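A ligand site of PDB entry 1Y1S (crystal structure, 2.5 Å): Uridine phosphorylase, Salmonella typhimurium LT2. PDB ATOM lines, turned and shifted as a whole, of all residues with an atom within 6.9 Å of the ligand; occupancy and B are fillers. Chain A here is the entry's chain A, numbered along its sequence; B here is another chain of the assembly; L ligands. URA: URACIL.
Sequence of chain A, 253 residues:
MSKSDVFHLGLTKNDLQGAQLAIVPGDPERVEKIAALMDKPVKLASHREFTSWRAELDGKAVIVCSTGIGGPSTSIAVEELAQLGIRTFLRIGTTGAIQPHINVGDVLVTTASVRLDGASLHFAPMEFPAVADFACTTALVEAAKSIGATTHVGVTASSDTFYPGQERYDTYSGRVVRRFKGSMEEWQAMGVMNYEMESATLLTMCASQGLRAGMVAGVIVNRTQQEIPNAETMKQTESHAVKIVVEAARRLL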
ATOM      1  N   ARG A  91     -24.274   3.267 -32.733  1.00  0.00           N
ATOM      2  CA  ARG A  91     -23.433   2.609 -31.761  1.00  0.00           C
ATOM      3  C   ARG A  91     -22.530   1.596 -32.455  1.00  0.00           C
ATOM      4  O   ARG A  91     -22.998   0.652 -33.104  1.00  0.00           O
ATOM      5  CB  ARG A  91     -24.321   1.861 -30.763  1.00  0.00           C
ATOM      6  CG  ARG A  91     -23.854   1.858 -29.324  1.00  0.00           C
ATOM      7  CD  ARG A  91     -22.502   1.202 -29.125  1.00  0.00           C
ATOM      8  NE  ARG A  91     -22.599  -0.063 -28.397  1.00  0.00           N
ATOM      9  CZ  ARG A  91     -21.605  -0.602 -27.703  1.00  0.00           C
ATOM     10  NH1 ARG A  91     -20.427   0.005 -27.613  1.00  0.00           N
ATOM     11  NH2 ARG A  91     -21.774  -1.786 -27.138  1.00  0.00           N
ATOM     12  N   THR A  94     -17.793  -3.561 -29.532  1.00  0.00           N
ATOM     13  CA  THR A  94     -17.220  -4.898 -29.611  1.00  0.00           C
ATOM     14  C   THR A  94     -18.172  -5.793 -28.820  1.00  0.00           C
ATOM     15  O   THR A  94     -18.925  -5.297 -27.978  1.00  0.00           O
ATOM     16  CB  THR A  94     -15.833  -4.961 -28.953  1.00  0.00           C
ATOM     17  OG1 THR A  94     -15.953  -4.579 -27.578  1.00  0.00           O
ATOM     18  CG2 THR A  94     -14.865  -4.034 -29.667  1.00  0.00           C
ATOM     19  N   THR A  95     -18.119  -7.103 -29.072  1.00  0.00           N
ATOM     20  CA  THR A  95     -19.017  -8.023 -28.402  1.00  0.00           C
ATOM     21  C   THR A  95     -18.515  -9.472 -28.349  1.00  0.00           C
ATOM     22  O   THR A  95     -17.534  -9.848 -29.001  1.00  0.00           O
ATOM     23  CB  THR A  95     -20.391  -8.023 -29.106  1.00  0.00           C
ATOM     24  OG1 THR A  95     -21.191  -9.104 -28.612  1.00  0.00           O
ATOM     25  CG2 THR A  95     -20.206  -8.174 -30.602  1.00  0.00           C
ATOM     26  N   GLY A  96     -19.200 -10.270 -27.530  1.00  0.00           N
ATOM     27  CA  GLY A  96     -18.852 -11.673 -27.380  1.00  0.00           C
ATOM     28  C   GLY A  96     -19.978 -12.478 -27.981  1.00  0.00           C
ATOM     29  O   GLY A  96     -21.082 -12.542 -27.421  1.00  0.00           O
ATOM     30  N   ALA A  97     -19.714 -13.070 -29.130  1.00  0.00           N
ATOM     31  CA  ALA A  97     -20.718 -13.869 -29.818  1.00  0.00           C
ATOM     32  C   ALA A  97     -21.021 -15.122 -28.999  1.00  0.00           C
ATOM     33  O   ALA A  97     -20.130 -15.651 -28.320  1.00  0.00           O
ATOM     34  CB  ALA A  97     -20.208 -14.244 -31.207  1.00  0.00           C
ATOM     35  N   ALA A 157     -28.020  -9.650 -26.532  1.00  0.00           N
ATOM     36  CA  ALA A 157     -28.180  -9.643 -25.087  1.00  0.00           C
ATOM     37  C   ALA A 157     -27.391  -8.454 -24.554  1.00  0.00           C
ATOM     38  O   ALA A 157     -26.171  -8.417 -24.678  1.00  0.00           O
ATOM     39  CB  ALA A 157     -27.645 -10.933 -24.495  1.00  0.00           C
ATOM     40  N   SER A 159     -26.289  -6.789 -21.362  1.00  0.00           N
ATOM     41  CA  SER A 159     -26.115  -6.919 -19.907  1.00  0.00           C
ATOM     42  C   SER A 159     -25.439  -5.740 -19.226  1.00  0.00           C
ATOM     43  O   SER A 159     -24.512  -5.141 -19.773  1.00  0.00           O
ATOM     44  CB  SER A 159     -25.313  -8.171 -19.583  1.00  0.00           C
ATOM     45  OG  SER A 159     -24.862  -8.131 -18.246  1.00  0.00           O
ATOM     46  N   THR A 161     -23.639  -5.995 -16.691  1.00  0.00           N
ATOM     47  CA  THR A 161     -22.370  -6.443 -16.160  1.00  0.00           C
ATOM     48  C   THR A 161     -21.626  -7.194 -17.244  1.00  0.00           C
ATOM     49  O   THR A 161     -22.196  -7.598 -18.247  1.00  0.00           O
ATOM     50  CB  THR A 161     -22.540  -7.390 -14.938  1.00  0.00           C
ATOM     51  OG1 THR A 161     -23.146  -8.625 -15.348  1.00  0.00           O
ATOM     52  CG2 THR A 161     -23.384  -6.717 -13.883  1.00  0.00           C
ATOM     53  N   PHE A 162     -20.328  -7.369 -17.026  1.00  0.00           N
ATOM     54  CA  PHE A 162     -19.485  -8.070 -17.979  1.00  0.00           C
ATOM     55  C   PHE A 162     -19.290  -9.517 -17.556  1.00  0.00           C
ATOM     56  O   PHE A 162     -18.978 -10.380 -18.387  1.00  0.00           O
ATOM     57  CB  PHE A 162     -18.135  -7.342 -18.068  1.00  0.00           C
ATOM     58  CG  PHE A 162     -17.150  -7.991 -19.013  1.00  0.00           C
ATOM     59  CD1 PHE A 162     -16.395  -9.096 -18.617  1.00  0.00           C
ATOM     60  CD2 PHE A 162     -16.987  -7.498 -20.312  1.00  0.00           C
ATOM     61  CE1 PHE A 162     -15.489  -9.700 -19.490  1.00  0.00           C
ATOM     62  CE2 PHE A 162     -16.080  -8.102 -21.186  1.00  0.00           C
ATOM     63  CZ  PHE A 162     -15.333  -9.210 -20.769  1.00  0.00           C
ATOM     64  N   GLN A 166     -23.402 -12.185 -17.903  1.00  0.00           N
ATOM     65  CA  GLN A 166     -23.011 -12.814 -19.157  1.00  0.00           C
ATOM     66  C   GLN A 166     -22.505 -14.182 -18.788  1.00  0.00           C
ATOM     67  O   GLN A 166     -21.635 -14.760 -19.450  1.00  0.00           O
ATOM     68  CB  GLN A 166     -21.900 -12.009 -19.840  1.00  0.00           C
ATOM     69  CG  GLN A 166     -22.337 -10.636 -20.273  1.00  0.00           C
ATOM     70  CD  GLN A 166     -21.287  -9.953 -21.126  1.00  0.00           C
ATOM     71  OE1 GLN A 166     -20.635 -10.590 -21.952  1.00  0.00           O
ATOM     72  NE2 GLN A 166     -21.138  -8.644 -20.936  1.00  0.00           N
ATOM     73  N   ARG A 168     -20.356 -15.492 -16.871  1.00  0.00           N
ATOM     74  CA  ARG A 168     -18.934 -15.820 -16.870  1.00  0.00           C
ATOM     75  C   ARG A 168     -18.664 -16.359 -15.462  1.00  0.00           C
ATOM     76  O   ARG A 168     -19.150 -15.795 -14.479  1.00  0.00           O
ATOM     77  CB  ARG A 168     -18.078 -14.572 -17.138  1.00  0.00           C
ATOM     78  CG  ARG A 168     -17.849 -14.266 -18.609  1.00  0.00           C
ATOM     79  CD  ARG A 168     -16.829 -13.151 -18.807  1.00  0.00           C
ATOM     80  NE  ARG A 168     -16.322 -13.112 -20.175  1.00  0.00           N
ATOM     81  CZ  ARG A 168     -16.790 -12.334 -21.147  1.00  0.00           C
ATOM     82  NH1 ARG A 168     -17.805 -11.512 -20.935  1.00  0.00           N
ATOM     83  NH2 ARG A 168     -16.249 -12.414 -22.357  1.00  0.00           N
ATOM     84  N   TYR A 195     -23.468 -10.801 -26.703  1.00  0.00           N
ATOM     85  CA  TYR A 195     -23.503 -10.038 -25.460  1.00  0.00           C
ATOM     86  C   TYR A 195     -22.745  -8.720 -25.627  1.00  0.00           C
ATOM     87  O   TYR A 195     -21.623  -8.711 -26.134  1.00  0.00           O
ATOM     88  CB  TYR A 195     -22.807 -10.807 -24.321  1.00  0.00           C
ATOM     89  CG  TYR A 195     -23.587 -11.914 -23.615  1.00  0.00           C
ATOM     90  CD1 TYR A 195     -24.744 -11.644 -22.875  1.00  0.00           C
ATOM     91  CD2 TYR A 195     -23.094 -13.228 -23.621  1.00  0.00           C
ATOM     92  CE1 TYR A 195     -25.382 -12.644 -22.145  1.00  0.00           C
ATOM     93  CE2 TYR A 195     -23.729 -14.238 -22.890  1.00  0.00           C
ATOM     94  CZ  TYR A 195     -24.862 -13.946 -22.153  1.00  0.00           C
ATOM     95  OH  TYR A 195     -25.442 -14.952 -21.395  1.00  0.00           O
ATOM     96  N   GLU A 196     -23.357  -7.624 -25.197  1.00  0.00           N
ATOM     97  CA  GLU A 196     -22.721  -6.320 -25.216  1.00  0.00           C
ATOM     98  C   GLU A 196     -23.343  -5.577 -24.028  1.00  0.00           C
ATOM     99  O   GLU A 196     -24.230  -6.121 -23.376  1.00  0.00           O
ATOM    100  CB  GLU A 196     -22.931  -5.611 -26.580  1.00  0.00           C
ATOM    101  CG  GLU A 196     -24.357  -5.303 -26.981  1.00  0.00           C
ATOM    102  CD  GLU A 196     -24.890  -4.084 -26.283  1.00  0.00           C
ATOM    103  OE1 GLU A 196     -24.254  -3.023 -26.375  1.00  0.00           O
ATOM    104  OE2 GLU A 196     -25.964  -4.175 -25.642  1.00  0.00           O
ATOM    105  N   MET A 197     -22.892  -4.360 -23.718  1.00  0.00           N
ATOM    106  CA  MET A 197     -23.401  -3.698 -22.520  1.00  0.00           C
ATOM    107  C   MET A 197     -24.047  -2.323 -22.580  1.00  0.00           C
ATOM    108  O   MET A 197     -24.103  -1.635 -21.571  1.00  0.00           O
ATOM    109  CB  MET A 197     -22.280  -3.652 -21.494  1.00  0.00           C
ATOM    110  CG  MET A 197     -21.722  -5.020 -21.148  1.00  0.00           C
ATOM    111  SD  MET A 197     -20.285  -4.889 -20.076  1.00  0.00           S
ATOM    112  CE  MET A 197     -21.005  -4.102 -18.674  1.00  0.00           C
ATOM    113  N   GLU A 198     -24.539  -1.902 -23.737  1.00  0.00           N
ATOM    114  CA  GLU A 198     -25.175  -0.599 -23.792  1.00  0.00           C
ATOM    115  C   GLU A 198     -26.267  -0.436 -24.835  1.00  0.00           C
ATOM    116  O   GLU A 198     -26.878   0.625 -24.925  1.00  0.00           O
ATOM    117  CB  GLU A 198     -24.115   0.501 -23.971  1.00  0.00           C
ATOM    118  CG  GLU A 198     -22.899   0.079 -24.785  1.00  0.00           C
ATOM    119  CD  GLU A 198     -21.793  -0.535 -23.942  1.00  0.00           C
ATOM    120  OE1 GLU A 198     -21.180  -1.532 -24.378  1.00  0.00           O
ATOM    121  OE2 GLU A 198     -21.526  -0.018 -22.839  1.00  0.00           O
ATOM    122  N   GLY A 218     -18.333  -5.581 -33.434  1.00  0.00           N
ATOM    123  CA  GLY A 218     -17.415  -6.569 -33.960  1.00  0.00           C
ATOM    124  C   GLY A 218     -17.166  -7.671 -32.952  1.00  0.00           C
ATOM    125  O   GLY A 218     -16.811  -7.398 -31.807  1.00  0.00           O
ATOM    126  N   ILE A 220     -15.308  -9.936 -30.971  1.00  0.00           N
ATOM    127  CA  ILE A 220     -13.918 -10.106 -30.548  1.00  0.00           C
ATOM    128  C   ILE A 220     -13.687 -11.425 -29.835  1.00  0.00           C
ATOM    129  O   ILE A 220     -12.553 -11.776 -29.494  1.00  0.00           O
ATOM    130  CB  ILE A 220     -13.427  -8.953 -29.613  1.00  0.00           C
ATOM    131  CG1 ILE A 220     -14.280  -8.896 -28.343  1.00  0.00           C
ATOM    132  CG2 ILE A 220     -13.458  -7.645 -30.347  1.00  0.00           C
ATOM    133  CD1 ILE A 220     -13.762  -7.913 -27.308  1.00  0.00           C
ATOM    134  N   VAL A 221     -14.766 -12.172 -29.619  1.00  0.00           N
ATOM    135  CA  VAL A 221     -14.661 -13.461 -28.952  1.00  0.00           C
ATOM    136  C   VAL A 221     -15.935 -14.288 -29.111  1.00  0.00           C
ATOM    137  O   VAL A 221     -17.027 -13.747 -29.277  1.00  0.00           O
ATOM    138  CB  VAL A 221     -14.341 -13.285 -27.436  1.00  0.00           C
ATOM    139  CG1 VAL A 221     -15.582 -12.767 -26.688  1.00  0.00           C
ATOM    140  CG2 VAL A 221     -13.888 -14.611 -26.837  1.00  0.00           C
ATOM    141  N   ARG A 223     -17.934 -17.213 -27.102  1.00  0.00           N
ATOM    142  CA  ARG A 223     -18.088 -17.967 -25.864  1.00  0.00           C
ATOM    143  C   ARG A 223     -18.276 -19.476 -25.988  1.00  0.00           C
ATOM    144  O   ARG A 223     -18.438 -20.156 -24.976  1.00  0.00           O
ATOM    145  CB  ARG A 223     -19.250 -17.369 -25.066  1.00  0.00           C
ATOM    146  CG  ARG A 223     -19.046 -15.897 -24.690  1.00  0.00           C
ATOM    147  CD  ARG A 223     -18.015 -15.777 -23.574  1.00  0.00           C
ATOM    148  NE  ARG A 223     -18.453 -16.550 -22.419  1.00  0.00           N
ATOM    149  CZ  ARG A 223     -19.474 -16.208 -21.651  1.00  0.00           C
ATOM    150  NH1 ARG A 223     -20.153 -15.097 -21.912  1.00  0.00           N
ATOM    151  NH2 ARG A 223     -19.854 -16.996 -20.670  1.00  0.00           N
ATOM    152  N   PHE B   7      -8.957  -8.200 -17.413  1.00  0.00           N
ATOM    153  CA  PHE B   7      -9.320  -7.842 -18.773  1.00  0.00           C
ATOM    154  C   PHE B   7      -9.421  -6.339 -19.104  1.00  0.00           C
ATOM    155  O   PHE B   7      -9.059  -5.991 -20.224  1.00  0.00           O
ATOM    156  CB  PHE B   7     -10.591  -8.540 -19.263  1.00  0.00           C
ATOM    157  CG  PHE B   7     -10.780  -8.463 -20.773  1.00  0.00           C
ATOM    158  CD1 PHE B   7     -10.046  -9.273 -21.642  1.00  0.00           C
ATOM    159  CD2 PHE B   7     -11.704  -7.581 -21.325  1.00  0.00           C
ATOM    160  CE1 PHE B   7     -10.239  -9.213 -23.031  1.00  0.00           C
ATOM    161  CE2 PHE B   7     -11.904  -7.502 -22.704  1.00  0.00           C
ATOM    162  CZ  PHE B   7     -11.165  -8.320 -23.553  1.00  0.00           C
ATOM    163  N   HIS B   8      -9.859  -5.410 -18.261  1.00  0.00           N
ATOM    164  CA  HIS B   8      -9.880  -4.034 -18.799  1.00  0.00           C
ATOM    165  C   HIS B   8      -8.945  -3.027 -18.131  1.00  0.00           C
ATOM    166  O   HIS B   8      -8.533  -2.032 -18.727  1.00  0.00           O
ATOM    167  CB  HIS B   8     -11.282  -3.453 -18.699  1.00  0.00           C
ATOM    168  CG  HIS B   8     -12.378  -4.389 -19.112  1.00  0.00           C
ATOM    169  ND1 HIS B   8     -12.662  -5.598 -18.477  1.00  0.00           N
ATOM    170  CD2 HIS B   8     -13.281  -4.305 -20.130  1.00  0.00           C
ATOM    171  CE1 HIS B   8     -13.682  -6.192 -19.079  1.00  0.00           C
ATOM    172  NE2 HIS B   8     -14.071  -5.425 -20.085  1.00  0.00           N
HETATM  173  N1  URA L   1     -17.880  -7.068 -24.840  1.00  0.00           N
HETATM  174  C2  URA L   1     -18.852  -7.630 -23.991  1.00  0.00           C
HETATM  175  O2  URA L   1     -19.696  -6.916 -23.481  1.00  0.00           O
HETATM  176  N3  URA L   1     -18.749  -9.019 -23.829  1.00  0.00           N
HETATM  177  C4  URA L   1     -17.778  -9.889 -24.416  1.00  0.00           C
HETATM  178  O4  URA L   1     -17.843 -11.074 -24.157  1.00  0.00           O
HETATM  179  C5  URA L   1     -16.814  -9.210 -25.272  1.00  0.00           C
HETATM  180  C6  URA L   1     -16.881  -7.882 -25.453  1.00  0.00           C
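The side-chain amide oxygen (OE1) of Gln 166 is in hydrogen-bond range of the guanidinium group (NH1) of Arg 168.
The side-chain amide nitrogen of Gln 166 is in hydrogen-bond range of the backbone carbonyl oxygen of Thr 161, at 3.1 Å.
The backbone carbonyl oxygen of Gly 96 sits at hydrogen-bond distance from the backbone NH of Tyr 195.
O of Thr 95 sits at hydrogen-bond distance from N of Ile 220.
The backbone carbonyl oxygen (O) of Tyr 195 lies within hydrogen-bond range of the side-chain hydroxyl (OG1) of Thr 95 (2.5 Å).
OE1 of Glu 196 lies within hydrogen-bond range of N of Glu 198, at 2.9 Å.
The backbone carbonyl oxygen of Glu 196 lies within hydrogen-bond range of the backbone NH of Ser 159 (3.0 Å).
NH2 of Arg 91 is in salt-bridge range of OE1 of Glu 196 (2.9 Å).
The guanidinium group (NH2) of Arg 168 lies within hydrogen-bond range of an oxygen (O4) of the ligand (2.8 Å).
OE1 of Gln 166 is in hydrogen-bond range of N3 of the ligand.
Thr 94 touches the ligand.
C of Thr 95 touches C5 of the ligand, at 3.5 Å.
Gly 96 touches the ligand.
CE2 of Phe 162 touches N3 of the ligand (3.9 Å).
Tyr 195 touches the ligand (O to C2, 3.7 Å).
Glu 196 touches the ligand (CA to O2, 3.5 Å).
Met 197 touches the ligand (CG to O2, 3.6 Å).
Ile 220 touches the ligand.
Val 221 touches the ligand.
Hydrophobic or aromatic side chains that line the ligand: Phe 162, Met 197, Ile 220 and Val 221.
11 residues have an atom within 4 Å of the ligand: Thr 94, Thr 95, Gly 96, Phe 162, Gln 166, Arg 168, Tyr 195, Glu 196, Met 197, Ile 220 and Val 221.
The nearest printed residue that does not touch the ligand is Arg 223 (4.7 Å).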
